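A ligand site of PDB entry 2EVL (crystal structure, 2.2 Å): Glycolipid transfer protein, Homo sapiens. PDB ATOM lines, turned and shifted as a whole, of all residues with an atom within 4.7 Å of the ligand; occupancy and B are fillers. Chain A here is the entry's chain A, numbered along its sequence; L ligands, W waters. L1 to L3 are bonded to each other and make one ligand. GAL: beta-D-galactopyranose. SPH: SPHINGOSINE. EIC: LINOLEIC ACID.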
ATOM      1  N   PHE A  34      -2.732 -11.344  21.518  1.00  0.00           N
ATOM      2  CA  PHE A  34      -3.117 -10.010  21.031  1.00  0.00           C
ATOM      3  C   PHE A  34      -2.446  -9.619  19.695  1.00  0.00           C
ATOM      4  O   PHE A  34      -2.917  -8.706  19.021  1.00  0.00           O
ATOM      5  CB  PHE A  34      -2.827  -8.929  22.076  1.00  0.00           C
ATOM      6  CG  PHE A  34      -3.795  -8.924  23.216  1.00  0.00           C
ATOM      7  CD1 PHE A  34      -5.025  -8.295  23.073  1.00  0.00           C
ATOM      8  CD2 PHE A  34      -3.500  -9.551  24.418  1.00  0.00           C
ATOM      9  CE1 PHE A  34      -5.926  -8.288  24.105  1.00  0.00           C
ATOM     10  CE2 PHE A  34      -4.408  -9.550  25.467  1.00  0.00           C
ATOM     11  CZ  PHE A  34      -5.610  -8.913  25.318  1.00  0.00           C
ATOM     12  N   LEU A  37      -5.143 -10.874  16.705  1.00  0.00           N
ATOM     13  CA  LEU A  37      -6.547 -10.436  16.596  1.00  0.00           C
ATOM     14  C   LEU A  37      -6.725  -9.533  15.401  1.00  0.00           C
ATOM     15  O   LEU A  37      -7.831  -9.063  15.127  1.00  0.00           O
ATOM     16  CB  LEU A  37      -7.001  -9.687  17.848  1.00  0.00           C
ATOM     17  CG  LEU A  37      -7.647 -10.515  18.947  1.00  0.00           C
ATOM     18  CD1 LEU A  37      -6.715 -11.638  19.383  1.00  0.00           C
ATOM     19  CD2 LEU A  37      -7.996  -9.625  20.115  1.00  0.00           C
ATOM     20  N   PHE A  42      -4.654  -3.245  19.150  1.00  0.00           N
ATOM     21  CA  PHE A  42      -4.370  -4.123  20.288  1.00  0.00           C
ATOM     22  C   PHE A  42      -2.961  -4.000  20.879  1.00  0.00           C
ATOM     23  O   PHE A  42      -2.662  -4.605  21.918  1.00  0.00           O
ATOM     24  CB  PHE A  42      -4.678  -5.572  19.910  1.00  0.00           C
ATOM     25  CG  PHE A  42      -6.134  -5.792  19.563  1.00  0.00           C
ATOM     26  CD1 PHE A  42      -7.109  -5.673  20.544  1.00  0.00           C
ATOM     27  CD2 PHE A  42      -6.525  -6.059  18.256  1.00  0.00           C
ATOM     28  CE1 PHE A  42      -8.447  -5.823  20.231  1.00  0.00           C
ATOM     29  CE2 PHE A  42      -7.876  -6.233  17.951  1.00  0.00           C
ATOM     30  CZ  PHE A  42      -8.831  -6.113  18.942  1.00  0.00           C
ATOM     31  N   PRO A  44      -1.316  -1.334  22.347  1.00  0.00           N
ATOM     32  CA  PRO A  44      -1.324  -0.712  23.663  1.00  0.00           C
ATOM     33  C   PRO A  44      -1.945  -1.580  24.736  1.00  0.00           C
ATOM     34  O   PRO A  44      -1.591  -1.495  25.899  1.00  0.00           O
ATOM     35  CB  PRO A  44      -2.197   0.545  23.458  1.00  0.00           C
ATOM     36  CG  PRO A  44      -2.194   0.767  22.006  1.00  0.00           C
ATOM     37  CD  PRO A  44      -2.159  -0.587  21.403  1.00  0.00           C
ATOM     38  N   ILE A  45      -2.924  -2.390  24.338  1.00  0.00           N
ATOM     39  CA  ILE A  45      -3.570  -3.334  25.254  1.00  0.00           C
ATOM     40  C   ILE A  45      -2.581  -4.397  25.727  1.00  0.00           C
ATOM     41  O   ILE A  45      -2.478  -4.660  26.932  1.00  0.00           O
ATOM     42  CB  ILE A  45      -4.786  -3.998  24.581  1.00  0.00           C
ATOM     43  CG1 ILE A  45      -5.932  -2.994  24.538  1.00  0.00           C
ATOM     44  CG2 ILE A  45      -5.214  -5.263  25.325  1.00  0.00           C
ATOM     45  CD1 ILE A  45      -7.094  -3.381  23.576  1.00  0.00           C
ATOM     46  N   ASP A  48      -0.132  -2.928  28.311  1.00  0.00           N
ATOM     47  CA  ASP A  48      -0.614  -2.730  29.678  1.00  0.00           C
ATOM     48  C   ASP A  48      -0.535  -4.036  30.465  1.00  0.00           C
ATOM     49  O   ASP A  48      -0.086  -4.041  31.602  1.00  0.00           O
ATOM     50  CB  ASP A  48      -2.065  -2.226  29.689  1.00  0.00           C
ATOM     51  CG  ASP A  48      -2.552  -1.969  31.076  1.00  0.00           C
ATOM     52  OD1 ASP A  48      -2.435  -0.804  31.526  1.00  0.00           O
ATOM     53  OD2 ASP A  48      -3.002  -2.927  31.740  1.00  0.00           O
ATOM     54  N   ILE A  49      -0.978  -5.115  29.839  1.00  0.00           N
ATOM     55  CA  ILE A  49      -1.004  -6.418  30.463  1.00  0.00           C
ATOM     56  C   ILE A  49       0.421  -6.888  30.720  1.00  0.00           C
ATOM     57  O   ILE A  49       0.766  -7.237  31.865  1.00  0.00           O
ATOM     58  CB  ILE A  49      -1.816  -7.472  29.618  1.00  0.00           C
ATOM     59  CG1 ILE A  49      -3.300  -7.022  29.524  1.00  0.00           C
ATOM     60  CG2 ILE A  49      -1.736  -8.811  30.288  1.00  0.00           C
ATOM     61  CD1 ILE A  49      -4.180  -7.799  28.637  1.00  0.00           C
ATOM     62  N   ASN A  52       2.326  -4.777  33.309  1.00  0.00           N
ATOM     63  CA  ASN A  52       1.960  -5.173  34.667  1.00  0.00           C
ATOM     64  C   ASN A  52       2.562  -6.492  35.085  1.00  0.00           C
ATOM     65  O   ASN A  52       3.036  -6.613  36.213  1.00  0.00           O
ATOM     66  CB  ASN A  52       0.442  -5.205  34.828  1.00  0.00           C
ATOM     67  CG  ASN A  52      -0.125  -3.833  35.006  1.00  0.00           C
ATOM     68  OD1 ASN A  52       0.488  -2.956  35.657  1.00  0.00           O
ATOM     69  ND2 ASN A  52      -1.326  -3.619  34.463  1.00  0.00           N
ATOM     70  N   LYS A  55       6.197  -5.694  35.853  1.00  0.00           N
ATOM     71  CA  LYS A  55       6.260  -5.034  37.170  1.00  0.00           C
ATOM     72  C   LYS A  55       6.168  -6.004  38.355  1.00  0.00           C
ATOM     73  O   LYS A  55       6.879  -5.848  39.360  1.00  0.00           O
ATOM     74  CB  LYS A  55       5.126  -3.996  37.308  1.00  0.00           C
ATOM     75  CG  LYS A  55       5.395  -2.678  36.604  1.00  0.00           C
ATOM     76  CD  LYS A  55       4.180  -1.758  36.673  1.00  0.00           C
ATOM     77  CE  LYS A  55       4.409  -0.444  35.950  1.00  0.00           C
ATOM     78  NZ  LYS A  55       3.185   0.010  35.208  1.00  0.00           N
ATOM     79  N   LEU A  92      -0.244  -2.509  43.025  1.00  0.00           N
ATOM     80  CA  LEU A  92      -0.945  -1.732  42.018  1.00  0.00           C
ATOM     81  C   LEU A  92      -0.951  -2.386  40.637  1.00  0.00           C
ATOM     82  O   LEU A  92      -1.985  -2.377  39.943  1.00  0.00           O
ATOM     83  CB  LEU A  92      -0.362  -0.317  41.939  1.00  0.00           C
ATOM     84  CG  LEU A  92      -1.057   0.660  40.987  1.00  0.00           C
ATOM     85  CD1 LEU A  92      -2.504   0.849  41.381  1.00  0.00           C
ATOM     86  CD2 LEU A  92      -0.309   1.989  41.021  1.00  0.00           C
ATOM     87  N   ALA A  93       0.200  -2.916  40.222  1.00  0.00           N
ATOM     88  CA  ALA A  93       0.298  -3.640  38.956  1.00  0.00           C
ATOM     89  C   ALA A  93      -0.690  -4.813  38.882  1.00  0.00           C
ATOM     90  O   ALA A  93      -1.378  -4.983  37.894  1.00  0.00           O
ATOM     91  CB  ALA A  93       1.717  -4.117  38.719  1.00  0.00           C
ATOM     92  N   TRP A  96      -4.412  -3.942  38.497  1.00  0.00           N
ATOM     93  CA  TRP A  96      -4.778  -3.700  37.138  1.00  0.00           C
ATOM     94  C   TRP A  96      -4.676  -4.970  36.284  1.00  0.00           C
ATOM     95  O   TRP A  96      -5.485  -5.159  35.373  1.00  0.00           O
ATOM     96  CB  TRP A  96      -3.971  -2.546  36.550  1.00  0.00           C
ATOM     97  CG  TRP A  96      -4.471  -1.216  37.035  1.00  0.00           C
ATOM     98  CD1 TRP A  96      -3.988  -0.475  38.074  1.00  0.00           C
ATOM     99  CD2 TRP A  96      -5.615  -0.505  36.543  1.00  0.00           C
ATOM    100  NE1 TRP A  96      -4.737   0.675  38.235  1.00  0.00           N
ATOM    101  CE2 TRP A  96      -5.736   0.676  37.309  1.00  0.00           C
ATOM    102  CE3 TRP A  96      -6.522  -0.733  35.503  1.00  0.00           C
ATOM    103  CZ2 TRP A  96      -6.733   1.617  37.066  1.00  0.00           C
ATOM    104  CZ3 TRP A  96      -7.495   0.189  35.264  1.00  0.00           C
ATOM    105  CH2 TRP A  96      -7.599   1.354  36.031  1.00  0.00           C
ATOM    106  N   GLY A 100      -7.592  -6.899  33.683  1.00  0.00           N
ATOM    107  CA  GLY A 100      -7.286  -7.402  32.352  1.00  0.00           C
ATOM    108  C   GLY A 100      -7.562  -8.889  32.219  1.00  0.00           C
ATOM    109  O   GLY A 100      -8.185  -9.334  31.250  1.00  0.00           O
ATOM    110  N   PHE A 103     -11.300  -9.373  32.326  1.00  0.00           N
ATOM    111  CA  PHE A 103     -11.828  -9.024  31.015  1.00  0.00           C
ATOM    112  C   PHE A 103     -11.772 -10.237  30.091  1.00  0.00           C
ATOM    113  O   PHE A 103     -12.792 -10.627  29.531  1.00  0.00           O
ATOM    114  CB  PHE A 103     -11.076  -7.873  30.343  1.00  0.00           C
ATOM    115  CG  PHE A 103     -11.654  -7.514  28.990  1.00  0.00           C
ATOM    116  CD1 PHE A 103     -12.584  -6.503  28.874  1.00  0.00           C
ATOM    117  CD2 PHE A 103     -11.291  -8.237  27.846  1.00  0.00           C
ATOM    118  CE1 PHE A 103     -13.129  -6.196  27.633  1.00  0.00           C
ATOM    119  CE2 PHE A 103     -11.852  -7.947  26.602  1.00  0.00           C
ATOM    120  CZ  PHE A 103     -12.759  -6.931  26.488  1.00  0.00           C
ATOM    121  N   PHE A 107     -15.051 -12.308  28.655  1.00  0.00           N
ATOM    122  CA  PHE A 107     -15.166 -12.405  27.214  1.00  0.00           C
ATOM    123  C   PHE A 107     -15.217 -13.860  26.720  1.00  0.00           C
ATOM    124  O   PHE A 107     -16.101 -14.246  25.944  1.00  0.00           O
ATOM    125  CB  PHE A 107     -13.986 -11.672  26.580  1.00  0.00           C
ATOM    126  CG  PHE A 107     -13.988 -11.674  25.076  1.00  0.00           C
ATOM    127  CD1 PHE A 107     -14.925 -10.944  24.373  1.00  0.00           C
ATOM    128  CD2 PHE A 107     -13.021 -12.400  24.361  1.00  0.00           C
ATOM    129  CE1 PHE A 107     -14.907 -10.920  22.946  1.00  0.00           C
ATOM    130  CE2 PHE A 107     -13.009 -12.384  22.975  1.00  0.00           C
ATOM    131  CZ  PHE A 107     -13.972 -11.643  22.264  1.00  0.00           C
ATOM    132  N   ILE A 124     -18.403 -10.363  17.631  1.00  0.00           N
ATOM    133  CA  ILE A 124     -18.099 -10.605  19.042  1.00  0.00           C
ATOM    134  C   ILE A 124     -18.256  -9.323  19.876  1.00  0.00           C
ATOM    135  O   ILE A 124     -17.708  -9.228  20.968  1.00  0.00           O
ATOM    136  CB  ILE A 124     -16.684 -11.196  19.249  1.00  0.00           C
ATOM    137  CG1 ILE A 124     -15.607 -10.207  18.771  1.00  0.00           C
ATOM    138  CG2 ILE A 124     -16.570 -12.543  18.546  1.00  0.00           C
ATOM    139  CD1 ILE A 124     -14.231 -10.835  18.515  1.00  0.00           C
ATOM    140  N   ALA A 128     -17.475  -8.752  23.947  1.00  0.00           N
ATOM    141  CA  ALA A 128     -16.495  -7.773  24.375  1.00  0.00           C
ATOM    142  C   ALA A 128     -17.108  -6.701  25.256  1.00  0.00           C
ATOM    143  O   ALA A 128     -16.543  -6.339  26.306  1.00  0.00           O
ATOM    144  CB  ALA A 128     -15.858  -7.148  23.159  1.00  0.00           C
ATOM    145  N   LEU A 136     -13.723  -3.614  33.487  1.00  0.00           N
ATOM    146  CA  LEU A 136     -12.945  -2.387  33.298  1.00  0.00           C
ATOM    147  C   LEU A 136     -13.721  -1.057  33.340  1.00  0.00           C
ATOM    148  O   LEU A 136     -13.223  -0.086  33.903  1.00  0.00           O
ATOM    149  CB  LEU A 136     -12.190  -2.462  31.964  1.00  0.00           C
ATOM    150  CG  LEU A 136     -11.102  -3.529  31.863  1.00  0.00           C
ATOM    151  CD1 LEU A 136     -10.661  -3.725  30.419  1.00  0.00           C
ATOM    152  CD2 LEU A 136      -9.913  -3.167  32.747  1.00  0.00           C
ATOM    153  N   HIS A 140     -12.753   3.487  34.078  1.00  0.00           N
ATOM    154  CA  HIS A 140     -12.424   4.397  32.991  1.00  0.00           C
ATOM    155  C   HIS A 140     -13.326   5.651  33.016  1.00  0.00           C
ATOM    156  O   HIS A 140     -14.555   5.549  33.132  1.00  0.00           O
ATOM    157  CB  HIS A 140     -12.585   3.693  31.648  1.00  0.00           C
ATOM    158  CG  HIS A 140     -11.597   2.593  31.430  1.00  0.00           C
ATOM    159  ND1 HIS A 140     -11.672   1.749  30.353  1.00  0.00           N
ATOM    160  CD2 HIS A 140     -10.520   2.206  32.153  1.00  0.00           C
ATOM    161  CE1 HIS A 140     -10.674   0.890  30.406  1.00  0.00           C
ATOM    162  NE2 HIS A 140      -9.958   1.145  31.485  1.00  0.00           N
ATOM    163  N   ILE A 147     -12.789   5.716  23.656  1.00  0.00           N
ATOM    164  CA  ILE A 147     -11.721   5.008  22.924  1.00  0.00           C
ATOM    165  C   ILE A 147     -12.020   3.506  22.811  1.00  0.00           C
ATOM    166  O   ILE A 147     -11.818   2.914  21.735  1.00  0.00           O
ATOM    167  CB  ILE A 147     -10.322   5.225  23.559  1.00  0.00           C
ATOM    168  CG1 ILE A 147      -9.916   6.704  23.481  1.00  0.00           C
ATOM    169  CG2 ILE A 147      -9.264   4.363  22.846  1.00  0.00           C
ATOM    170  CD1 ILE A 147      -8.664   7.061  24.298  1.00  0.00           C
ATOM    171  N   PHE A 148     -12.509   2.890  23.888  1.00  0.00           N
ATOM    172  CA  PHE A 148     -12.945   1.495  23.810  1.00  0.00           C
ATOM    173  C   PHE A 148     -14.020   1.275  22.742  1.00  0.00           C
ATOM    174  O   PHE A 148     -13.963   0.321  21.964  1.00  0.00           O
ATOM    175  CB  PHE A 148     -13.492   0.987  25.136  1.00  0.00           C
ATOM    176  CG  PHE A 148     -14.251  -0.304  25.006  1.00  0.00           C
ATOM    177  CD1 PHE A 148     -13.575  -1.503  24.840  1.00  0.00           C
ATOM    178  CD2 PHE A 148     -15.649  -0.302  24.968  1.00  0.00           C
ATOM    179  CE1 PHE A 148     -14.271  -2.690  24.674  1.00  0.00           C
ATOM    180  CE2 PHE A 148     -16.351  -1.501  24.807  1.00  0.00           C
ATOM    181  CZ  PHE A 148     -15.660  -2.695  24.672  1.00  0.00           C
ATOM    182  N   ALA A 151     -12.317   1.210  19.461  1.00  0.00           N
ATOM    183  CA  ALA A 151     -11.484   0.002  19.352  1.00  0.00           C
ATOM    184  C   ALA A 151     -12.303  -1.280  19.139  1.00  0.00           C
ATOM    185  O   ALA A 151     -11.788  -2.251  18.589  1.00  0.00           O
ATOM    186  CB  ALA A 151     -10.620  -0.138  20.606  1.00  0.00           C
ATOM    187  N   LEU A 152     -13.554  -1.264  19.582  1.00  0.00           N
ATOM    188  CA  LEU A 152     -14.428  -2.434  19.469  1.00  0.00           C
ATOM    189  C   LEU A 152     -14.656  -2.827  18.014  1.00  0.00           C
ATOM    190  O   LEU A 152     -14.873  -3.991  17.706  1.00  0.00           O
ATOM    191  CB  LEU A 152     -15.764  -2.154  20.159  1.00  0.00           C
ATOM    192  CG  LEU A 152     -16.810  -3.251  20.261  1.00  0.00           C
ATOM    193  CD1 LEU A 152     -16.291  -4.456  21.022  1.00  0.00           C
ATOM    194  CD2 LEU A 152     -18.044  -2.693  20.940  1.00  0.00           C
ATOM    195  N   ALA A 155     -12.394  -5.543  16.443  1.00  0.00           N
ATOM    196  CA  ALA A 155     -12.695  -6.943  16.751  1.00  0.00           C
ATOM    197  C   ALA A 155     -12.948  -7.765  15.484  1.00  0.00           C
ATOM    198  O   ALA A 155     -13.726  -7.356  14.616  1.00  0.00           O
ATOM    199  CB  ALA A 155     -13.893  -7.021  17.660  1.00  0.00           C
ATOM    200  N   TYR A 207     -10.365   4.488  41.757  1.00  0.00           N
ATOM    201  CA  TYR A 207     -10.062   5.662  40.979  1.00  0.00           C
ATOM    202  C   TYR A 207     -10.214   5.330  39.502  1.00  0.00           C
ATOM    203  O   TYR A 207      -9.962   4.188  39.080  1.00  0.00           O
ATOM    204  CB  TYR A 207      -8.681   6.224  41.317  1.00  0.00           C
ATOM    205  CG  TYR A 207      -7.502   5.428  40.802  1.00  0.00           C
ATOM    206  CD1 TYR A 207      -6.934   5.725  39.569  1.00  0.00           C
ATOM    207  CD2 TYR A 207      -6.945   4.400  41.554  1.00  0.00           C
ATOM    208  CE1 TYR A 207      -5.860   5.005  39.092  1.00  0.00           C
ATOM    209  CE2 TYR A 207      -5.862   3.677  41.080  1.00  0.00           C
ATOM    210  CZ  TYR A 207      -5.322   3.990  39.852  1.00  0.00           C
ATOM    211  OH  TYR A 207      -4.228   3.290  39.369  1.00  0.00           O
ATOM    212  N   VAL A 209      -9.440   6.309  35.315  1.00  0.00           N
ATOM    213  CA  VAL A 209      -8.344   6.816  34.487  1.00  0.00           C
ATOM    214  C   VAL A 209      -8.817   7.629  33.296  1.00  0.00           C
ATOM    215  O   VAL A 209      -9.868   7.409  32.658  1.00  0.00           O
ATOM    216  CB  VAL A 209      -7.343   5.697  34.023  1.00  0.00           C
ATOM    217  CG1 VAL A 209      -6.478   5.224  35.210  1.00  0.00           C
ATOM    218  CG2 VAL A 209      -8.057   4.517  33.386  1.00  0.00           C
ATOM    219  OXT VAL A 209      -8.132   8.580  32.948  1.00  0.00           O
HETATM  220  C1  GAL L   1      -2.724   1.214  34.755  1.00  0.00           C
HETATM  221  C2  GAL L   1      -1.511   0.308  34.564  1.00  0.00           C
HETATM  222  C3  GAL L   1      -0.761   0.218  35.889  1.00  0.00           C
HETATM  223  C4  GAL L   1      -0.456   1.606  36.486  1.00  0.00           C
HETATM  224  C5  GAL L   1      -1.766   2.372  36.592  1.00  0.00           C
HETATM  225  C6  GAL L   1      -1.560   3.780  37.175  1.00  0.00           C
HETATM  226  O1  GAL L   1      -3.396   1.408  33.529  1.00  0.00           O
HETATM  227  O2  GAL L   1      -1.963  -0.979  34.135  1.00  0.00           O
HETATM  228  O3  GAL L   1       0.406  -0.540  35.744  1.00  0.00           O
HETATM  229  O4  GAL L   1       0.446   2.324  35.649  1.00  0.00           O
HETATM  230  O5  GAL L   1      -2.393   2.467  35.314  1.00  0.00           O
HETATM  231  O6  GAL L   1      -2.853   4.251  37.502  1.00  0.00           O
HETATM  232  C1  SPH L   2      -4.654   1.913  33.466  1.00  0.00           C
HETATM  233  C2  SPH L   2      -5.393   1.513  32.205  1.00  0.00           C
HETATM  234  N2  SPH L   2      -5.530   0.073  32.189  1.00  0.00           N
HETATM  235  C3  SPH L   2      -4.649   2.068  30.988  1.00  0.00           C
HETATM  236  O3  SPH L   2      -4.702   3.497  31.099  1.00  0.00           O
HETATM  237  C4  SPH L   2      -5.285   1.691  29.678  1.00  0.00           C
HETATM  238  C5  SPH L   2      -4.659   0.892  28.814  1.00  0.00           C
HETATM  239  C6  SPH L   2      -5.319   0.577  27.481  1.00  0.00           C
HETATM  240  C7  SPH L   2      -4.909   1.676  26.480  1.00  0.00           C
HETATM  241  C8  SPH L   2      -5.905   2.848  26.418  1.00  0.00           C
HETATM  242  C9  SPH L   2      -5.277   4.191  26.065  1.00  0.00           C
HETATM  243  C10 SPH L   2      -5.710   4.667  24.682  1.00  0.00           C
HETATM  244  C11 SPH L   2      -5.072   5.983  24.265  1.00  0.00           C
HETATM  245  C12 SPH L   2      -4.679   6.003  22.776  1.00  0.00           C
HETATM  246  C13 SPH L   2      -4.506   7.421  22.218  1.00  0.00           C
HETATM  247  C14 SPH L   2      -4.119   7.371  20.735  1.00  0.00           C
HETATM  248  C15 SPH L   2      -3.929   8.749  20.111  1.00  0.00           C
HETATM  249  C16 SPH L   2      -4.526   8.909  18.708  1.00  0.00           C
HETATM  250  C17 SPH L   2      -3.598   8.362  17.624  1.00  0.00           C
HETATM  251  C18 SPH L   2      -2.605   9.409  17.163  1.00  0.00           C
HETATM  252  C1  EIC L   3      -6.147  -1.039  31.972  1.00  0.00           C
HETATM  253  C2  EIC L   3      -6.298  -2.542  31.740  1.00  0.00           C
HETATM  254  C3  EIC L   3      -6.283  -2.844  30.234  1.00  0.00           C
HETATM  255  C4  EIC L   3      -6.719  -4.272  29.899  1.00  0.00           C
HETATM  256  C5  EIC L   3      -7.539  -4.274  28.611  1.00  0.00           C
HETATM  257  C6  EIC L   3      -8.128  -5.633  28.208  1.00  0.00           C
HETATM  258  C7  EIC L   3      -8.763  -5.472  26.823  1.00  0.00           C
HETATM  259  C8  EIC L   3      -8.579  -6.721  25.980  1.00  0.00           C
HETATM  260  C9  EIC L   3      -9.126  -6.735  24.558  1.00  0.00           C
HETATM  261  C10 EIC L   3      -9.848  -5.815  23.874  1.00  0.00           C
HETATM  262  C11 EIC L   3     -10.340  -4.454  24.339  1.00  0.00           C
HETATM  263  C12 EIC L   3     -10.599  -3.548  23.154  1.00  0.00           C
HETATM  264  C13 EIC L   3     -11.599  -3.710  22.281  1.00  0.00           C
HETATM  265  C14 EIC L   3     -12.635  -4.816  22.374  1.00  0.00           C
HETATM  266  C15 EIC L   3     -12.345  -5.900  21.327  1.00  0.00           C
HETATM  267  C16 EIC L   3     -12.391  -7.315  21.911  1.00  0.00           C
HETATM  268  C17 EIC L   3     -11.634  -8.343  21.055  1.00  0.00           C
HETATM  269  C18 EIC L   3     -11.209  -9.535  21.882  1.00  0.00           C
HETATM  270  O1  EIC L   3      -7.458  -0.432  32.029  1.00  0.00           O
HETATM  271  O   HOH W   1       0.346   2.852  32.903  1.00  0.00           O
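ND2 of Asn 52 sits at hydrogen-bond distance from O of Asp 48, at 3.1 Å.
The side-chain hydroxyl of Tyr 207 sits at hydrogen-bond distance from the indole nitrogen of Trp 96.
Residues that only touch the ligand: Phe 34, Leu 37, Phe 42, Ile 45, Trp 96, Phe 103, Phe 107, Ala 128, Leu 136, Ile 147, Phe 148, Ala 151 and Leu 152.
18 residues have an atom within 4 Å of the ligand: Phe 34, Leu 37, Phe 42, Ile 45, Asp 48, Asn 52, Lys 55, Trp 96, Phe 103, Phe 107, Ala 128, Leu 136, His 140, Ile 147, Phe 148, Ala 151, Leu 152 and Tyr 207.
NZ of Lys 55 is in hydrogen-bond range of O3 of GAL L1, 2.9 Å away.
OH of Tyr 207 lies within hydrogen-bond range of O6 of GAL L1 (2.5 Å).
OD1 of Asp 48 lies within hydrogen-bond range of O2 of GAL L1.
The side-chain amide oxygen (OD1) of Asn 52 is in hydrogen-bond range of an oxygen (O3) of GAL L1, 2.4 Å away.
A ring nitrogen (NE2) of His 140 is in hydrogen-bond range of an oxygen (O1) of EIC L3, at 3.0 Å.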
